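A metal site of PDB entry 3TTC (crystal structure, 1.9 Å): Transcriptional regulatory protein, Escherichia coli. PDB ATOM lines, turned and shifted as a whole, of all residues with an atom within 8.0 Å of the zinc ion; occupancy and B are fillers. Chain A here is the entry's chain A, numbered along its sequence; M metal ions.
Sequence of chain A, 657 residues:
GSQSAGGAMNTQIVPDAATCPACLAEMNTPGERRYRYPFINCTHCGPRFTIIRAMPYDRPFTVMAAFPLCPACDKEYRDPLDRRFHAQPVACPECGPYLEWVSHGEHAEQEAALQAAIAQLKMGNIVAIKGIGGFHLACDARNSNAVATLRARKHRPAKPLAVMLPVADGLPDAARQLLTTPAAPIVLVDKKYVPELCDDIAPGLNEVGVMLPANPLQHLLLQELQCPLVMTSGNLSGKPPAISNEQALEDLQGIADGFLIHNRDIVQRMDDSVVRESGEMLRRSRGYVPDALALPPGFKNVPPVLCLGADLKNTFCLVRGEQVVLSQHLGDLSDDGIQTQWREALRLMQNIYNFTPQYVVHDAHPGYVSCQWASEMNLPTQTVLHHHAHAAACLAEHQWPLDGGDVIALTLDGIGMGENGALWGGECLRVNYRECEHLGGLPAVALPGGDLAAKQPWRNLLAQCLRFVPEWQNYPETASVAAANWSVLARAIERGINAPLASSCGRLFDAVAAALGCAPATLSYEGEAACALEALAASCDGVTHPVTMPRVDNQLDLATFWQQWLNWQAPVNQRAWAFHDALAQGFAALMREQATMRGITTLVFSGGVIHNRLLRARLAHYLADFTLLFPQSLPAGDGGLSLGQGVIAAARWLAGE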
ATOM      1  N   ARG A  33       7.760   4.699   5.036  1.00  0.00           N
ATOM      2  CA  ARG A  33       7.553   5.601   3.895  1.00  0.00           C
ATOM      3  C   ARG A  33       7.074   6.992   4.348  1.00  0.00           C
ATOM      4  O   ARG A  33       7.413   8.002   3.743  1.00  0.00           O
ATOM      5  CB  ARG A  33       6.537   5.026   2.900  1.00  0.00           C
ATOM      6  CG  ARG A  33       6.400   5.819   1.596  1.00  0.00           C
ATOM      7  CD  ARG A  33       5.640   5.023   0.508  1.00  0.00           C
ATOM      8  NE  ARG A  33       4.179   5.212   0.563  1.00  0.00           N
ATOM      9  CZ  ARG A  33       3.326   4.388   1.169  1.00  0.00           C
ATOM     10  NH1 ARG A  33       3.762   3.301   1.794  1.00  0.00           N
ATOM     11  NH2 ARG A  33       2.024   4.654   1.145  1.00  0.00           N
ATOM     12  N   ARG A  34       6.275   7.018   5.418  1.00  0.00           N
ATOM     13  CA  ARG A  34       5.736   8.261   5.938  1.00  0.00           C
ATOM     14  C   ARG A  34       6.539   8.837   7.103  1.00  0.00           C
ATOM     15  O   ARG A  34       6.045   9.670   7.864  1.00  0.00           O
ATOM     16  CB  ARG A  34       4.255   8.098   6.301  1.00  0.00           C
ATOM     17  CG  ARG A  34       3.343   7.888   5.100  1.00  0.00           C
ATOM     18  CD  ARG A  34       1.888   7.869   5.500  1.00  0.00           C
ATOM     19  NE  ARG A  34       1.029   7.532   4.379  1.00  0.00           N
ATOM     20  CZ  ARG A  34       0.663   6.308   4.039  1.00  0.00           C
ATOM     21  NH1 ARG A  34      -0.120   6.121   2.971  1.00  0.00           N
ATOM     22  NH2 ARG A  34       1.084   5.268   4.741  1.00  0.00           N
ATOM     23  N   TYR A  37       6.620  12.619   7.684  1.00  0.00           N
ATOM     24  CA  TYR A  37       5.721  13.223   6.708  1.00  0.00           C
ATOM     25  C   TYR A  37       4.588  13.987   7.415  1.00  0.00           C
ATOM     26  O   TYR A  37       3.812  13.374   8.128  1.00  0.00           O
ATOM     27  CB  TYR A  37       5.132  12.175   5.765  1.00  0.00           C
ATOM     28  CG  TYR A  37       4.339  12.823   4.667  1.00  0.00           C
ATOM     29  CD1 TYR A  37       4.899  13.843   3.896  1.00  0.00           C
ATOM     30  CD2 TYR A  37       3.019  12.435   4.409  1.00  0.00           C
ATOM     31  CE1 TYR A  37       4.177  14.463   2.885  1.00  0.00           C
ATOM     32  CE2 TYR A  37       2.290  13.036   3.384  1.00  0.00           C
ATOM     33  CZ  TYR A  37       2.880  14.051   2.633  1.00  0.00           C
ATOM     34  OH  TYR A  37       2.165  14.660   1.633  1.00  0.00           O
ATOM     35  N   ARG A  59     -12.474  11.188  -2.208  1.00  0.00           N
ATOM     36  CA  ARG A  59     -11.289  11.974  -2.600  1.00  0.00           C
ATOM     37  C   ARG A  59     -11.470  12.985  -3.776  1.00  0.00           C
ATOM     38  O   ARG A  59     -10.963  14.121  -3.682  1.00  0.00           O
ATOM     39  CB  ARG A  59     -10.085  11.041  -2.820  1.00  0.00           C
ATOM     40  CG  ARG A  59      -8.757  11.781  -2.982  1.00  0.00           C
ATOM     41  CD  ARG A  59      -7.631  10.772  -3.206  1.00  0.00           C
ATOM     42  NE  ARG A  59      -6.323  11.406  -3.325  1.00  0.00           N
ATOM     43  CZ  ARG A  59      -5.458  11.590  -2.328  1.00  0.00           C
ATOM     44  NH1 ARG A  59      -5.756  11.202  -1.087  1.00  0.00           N
ATOM     45  NH2 ARG A  59      -4.292  12.179  -2.566  1.00  0.00           N
ATOM     46  N   PHE A  67      -3.885  15.471  -6.016  1.00  0.00           N
ATOM     47  CA  PHE A  67      -2.701  14.721  -5.648  1.00  0.00           C
ATOM     48  C   PHE A  67      -2.978  13.231  -5.900  1.00  0.00           C
ATOM     49  O   PHE A  67      -3.321  12.496  -4.982  1.00  0.00           O
ATOM     50  CB  PHE A  67      -2.368  14.918  -4.171  1.00  0.00           C
ATOM     51  CG  PHE A  67      -2.003  16.318  -3.788  1.00  0.00           C
ATOM     52  CD1 PHE A  67      -0.684  16.750  -3.853  1.00  0.00           C
ATOM     53  CD2 PHE A  67      -2.968  17.188  -3.293  1.00  0.00           C
ATOM     54  CE1 PHE A  67      -0.345  18.051  -3.461  1.00  0.00           C
ATOM     55  CE2 PHE A  67      -2.634  18.481  -2.896  1.00  0.00           C
ATOM     56  CZ  PHE A  67      -1.325  18.914  -2.991  1.00  0.00           C
ATOM     57  N   PRO A  68      -2.859  12.771  -7.164  1.00  0.00           N
ATOM     58  CA  PRO A  68      -3.084  11.349  -7.430  1.00  0.00           C
ATOM     59  C   PRO A  68      -2.158  10.451  -6.607  1.00  0.00           C
ATOM     60  O   PRO A  68      -0.962  10.739  -6.475  1.00  0.00           O
ATOM     61  CB  PRO A  68      -2.798  11.196  -8.930  1.00  0.00           C
ATOM     62  CG  PRO A  68      -2.098  12.470  -9.345  1.00  0.00           C
ATOM     63  CD  PRO A  68      -2.555  13.531  -8.389  1.00  0.00           C
ATOM     64  N   LEU A  69      -2.708   9.371  -6.063  1.00  0.00           N
ATOM     65  CA  LEU A  69      -1.985   8.488  -5.164  1.00  0.00           C
ATOM     66  C   LEU A  69      -0.902   7.688  -5.891  1.00  0.00           C
ATOM     67  O   LEU A  69      -1.144   7.182  -6.994  1.00  0.00           O
ATOM     68  CB  LEU A  69      -2.938   7.501  -4.488  1.00  0.00           C
ATOM     69  CG  LEU A  69      -3.966   8.053  -3.491  1.00  0.00           C
ATOM     70  CD1 LEU A  69      -4.684   6.917  -2.822  1.00  0.00           C
ATOM     71  CD2 LEU A  69      -3.284   8.919  -2.451  1.00  0.00           C
ATOM     72  N   CYS A  70       0.269   7.567  -5.275  1.00  0.00           N
ATOM     73  CA  CYS A  70       1.311   6.640  -5.762  1.00  0.00           C
ATOM     74  C   CYS A  70       0.792   5.208  -5.582  1.00  0.00           C
ATOM     75  O   CYS A  70      -0.207   4.993  -4.884  1.00  0.00           O
ATOM     76  CB  CYS A  70       2.628   6.862  -5.000  1.00  0.00           C
ATOM     77  SG  CYS A  70       2.604   6.315  -3.249  1.00  0.00           S
ATOM     78  N   PRO A  71       1.436   4.205  -6.234  1.00  0.00           N
ATOM     79  CA  PRO A  71       0.961   2.820  -6.082  1.00  0.00           C
ATOM     80  C   PRO A  71       0.872   2.313  -4.639  1.00  0.00           C
ATOM     81  O   PRO A  71      -0.076   1.596  -4.308  1.00  0.00           O
ATOM     82  CB  PRO A  71       2.003   2.013  -6.878  1.00  0.00           C
ATOM     83  CG  PRO A  71       2.508   2.988  -7.913  1.00  0.00           C
ATOM     84  CD  PRO A  71       2.562   4.298  -7.182  1.00  0.00           C
ATOM     85  N   ALA A  72       1.821   2.672  -3.790  1.00  0.00           N
ATOM     86  CA  ALA A  72       1.843   2.138  -2.427  1.00  0.00           C
ATOM     87  C   ALA A  72       0.678   2.684  -1.589  1.00  0.00           C
ATOM     88  O   ALA A  72       0.056   1.940  -0.806  1.00  0.00           O
ATOM     89  CB  ALA A  72       3.177   2.419  -1.764  1.00  0.00           C
ATOM     90  N   CYS A  73       0.386   3.978  -1.763  1.00  0.00           N
ATOM     91  CA  CYS A  73      -0.715   4.623  -1.062  1.00  0.00           C
ATOM     92  C   CYS A  73      -2.036   4.082  -1.596  1.00  0.00           C
ATOM     93  O   CYS A  73      -2.974   3.869  -0.838  1.00  0.00           O
ATOM     94  CB  CYS A  73      -0.676   6.144  -1.255  1.00  0.00           C
ATOM     95  SG  CYS A  73       0.515   7.042  -0.219  1.00  0.00           S
ATOM     96  N   ASP A  74      -2.089   3.880  -2.898  1.00  0.00           N
ATOM     97  CA  ASP A  74      -3.300   3.376  -3.518  1.00  0.00           C
ATOM     98  C   ASP A  74      -3.670   1.975  -3.004  1.00  0.00           C
ATOM     99  O   ASP A  74      -4.825   1.714  -2.667  1.00  0.00           O
ATOM    100  CB  ASP A  74      -3.172   3.408  -5.030  1.00  0.00           C
ATOM    101  CG  ASP A  74      -4.475   3.077  -5.720  1.00  0.00           C
ATOM    102  OD1 ASP A  74      -5.467   3.813  -5.538  1.00  0.00           O
ATOM    103  OD2 ASP A  74      -4.494   2.063  -6.441  1.00  0.00           O
ATOM    104  N   GLU A  76      -2.850   0.720  -0.095  1.00  0.00           N
ATOM    105  CA  GLU A  76      -3.306   0.845   1.285  1.00  0.00           C
ATOM    106  C   GLU A  76      -4.755   1.362   1.318  1.00  0.00           C
ATOM    107  O   GLU A  76      -5.602   0.819   2.050  1.00  0.00           O
ATOM    108  CB  GLU A  76      -2.338   1.717   2.112  1.00  0.00           C
ATOM    109  CG  GLU A  76      -0.958   1.034   2.335  1.00  0.00           C
ATOM    110  CD  GLU A  76       0.194   1.995   2.672  1.00  0.00           C
ATOM    111  OE1 GLU A  76      -0.039   3.180   2.962  1.00  0.00           O
ATOM    112  OE2 GLU A  76       1.363   1.543   2.638  1.00  0.00           O
ATOM    113  N   VAL A  90      -5.535  10.700   2.380  1.00  0.00           N
ATOM    114  CA  VAL A  90      -4.253   9.985   2.586  1.00  0.00           C
ATOM    115  C   VAL A  90      -3.165  10.422   1.592  1.00  0.00           C
ATOM    116  O   VAL A  90      -3.472  10.789   0.443  1.00  0.00           O
ATOM    117  CB  VAL A  90      -4.452   8.436   2.522  1.00  0.00           C
ATOM    118  CG1 VAL A  90      -4.820   7.954   1.091  1.00  0.00           C
ATOM    119  CG2 VAL A  90      -3.217   7.698   3.060  1.00  0.00           C
ATOM    120  N   ALA A  91      -1.917  10.410   2.036  1.00  0.00           N
ATOM    121  CA  ALA A  91      -0.806  10.754   1.187  1.00  0.00           C
ATOM    122  C   ALA A  91       0.538  10.289   1.771  1.00  0.00           C
ATOM    123  O   ALA A  91       0.619   9.875   2.921  1.00  0.00           O
ATOM    124  CB  ALA A  91      -0.784  12.266   0.924  1.00  0.00           C
ATOM    125  N   CYS A  92       1.589  10.333   0.964  1.00  0.00           N
ATOM    126  CA  CYS A  92       2.948  10.143   1.468  1.00  0.00           C
ATOM    127  C   CYS A  92       3.868  11.168   0.799  1.00  0.00           C
ATOM    128  O   CYS A  92       3.404  11.938  -0.047  1.00  0.00           O
ATOM    129  CB  CYS A  92       3.408   8.703   1.208  1.00  0.00           C
ATOM    130  SG  CYS A  92       3.931   8.371  -0.506  1.00  0.00           S
ATOM    131  N   PRO A  93       5.152  11.221   1.191  1.00  0.00           N
ATOM    132  CA  PRO A  93       6.056  12.198   0.557  1.00  0.00           C
ATOM    133  C   PRO A  93       6.127  12.120  -0.973  1.00  0.00           C
ATOM    134  O   PRO A  93       6.321  13.151  -1.620  1.00  0.00           O
ATOM    135  CB  PRO A  93       7.410  11.884   1.197  1.00  0.00           C
ATOM    136  CG  PRO A  93       7.040  11.353   2.582  1.00  0.00           C
ATOM    137  CD  PRO A  93       5.825  10.479   2.278  1.00  0.00           C
ATOM    138  N   GLU A  94       5.934  10.930  -1.530  1.00  0.00           N
ATOM    139  CA  GLU A  94       6.037  10.738  -2.997  1.00  0.00           C
ATOM    140  C   GLU A  94       4.843  11.280  -3.773  1.00  0.00           C
ATOM    141  O   GLU A  94       4.978  11.614  -4.963  1.00  0.00           O
ATOM    142  CB  GLU A  94       6.226   9.258  -3.328  1.00  0.00           C
ATOM    143  CG  GLU A  94       7.436   8.643  -2.646  1.00  0.00           C
ATOM    144  CD  GLU A  94       8.679   9.510  -2.821  1.00  0.00           C
ATOM    145  OE1 GLU A  94       9.088   9.745  -3.985  1.00  0.00           O
ATOM    146  OE2 GLU A  94       9.231   9.950  -1.793  1.00  0.00           O
ATOM    147  N   CYS A  95       3.675  11.340  -3.144  1.00  0.00           N
ATOM    148  CA  CYS A  95       2.465  11.754  -3.885  1.00  0.00           C
ATOM    149  C   CYS A  95       1.700  12.925  -3.297  1.00  0.00           C
ATOM    150  O   CYS A  95       0.814  13.456  -3.962  1.00  0.00           O
ATOM    151  CB  CYS A  95       1.519  10.572  -4.095  1.00  0.00           C
ATOM    152  SG  CYS A  95       0.822   9.866  -2.566  1.00  0.00           S
ATOM    153  N   GLY A  96       2.033  13.338  -2.087  1.00  0.00           N
ATOM    154  CA  GLY A  96       1.194  14.295  -1.381  1.00  0.00           C
ATOM    155  C   GLY A  96       1.729  15.717  -1.317  1.00  0.00           C
ATOM    156  O   GLY A  96       2.763  16.025  -1.943  1.00  0.00           O
HETATM  157 ZN    ZN M   1       1.935   7.997  -1.690  1.00  0.00          ZN
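The side-chain sulfur (SG) of Cys 70 sits close to the backbone NH (N) of Ala 72, 3.8 Å away.
SG of Cys 73 sits close to NH2 of Arg 33, at 3.1 Å.
OH of Tyr 37 lies within hydrogen-bond range of O of Cys 92 (3.4 Å).
SG of Cys 73 lies close to NH1 of Arg 34.
N of Glu 94 lies close to SG of Cys 92, at 3.4 Å.
NE of Arg 33 sits close to SG of Cys 92 (3.3 Å).
SG of Cys 73 binds the zinc ion, at 2.3 Å.
The side-chain sulfur (SG) of Cys 95 is bound to the zinc ion (2.3 Å).
The zinc ion is bound by SG of Cys 92 (2.4 Å).
The side-chain sulfur (SG) of Cys 70 is bound to the zinc ion, at 2.4 Å.
Within 4 Å of the zinc ion: Cys 70, Cys 73, Cys 92 and Cys 95.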
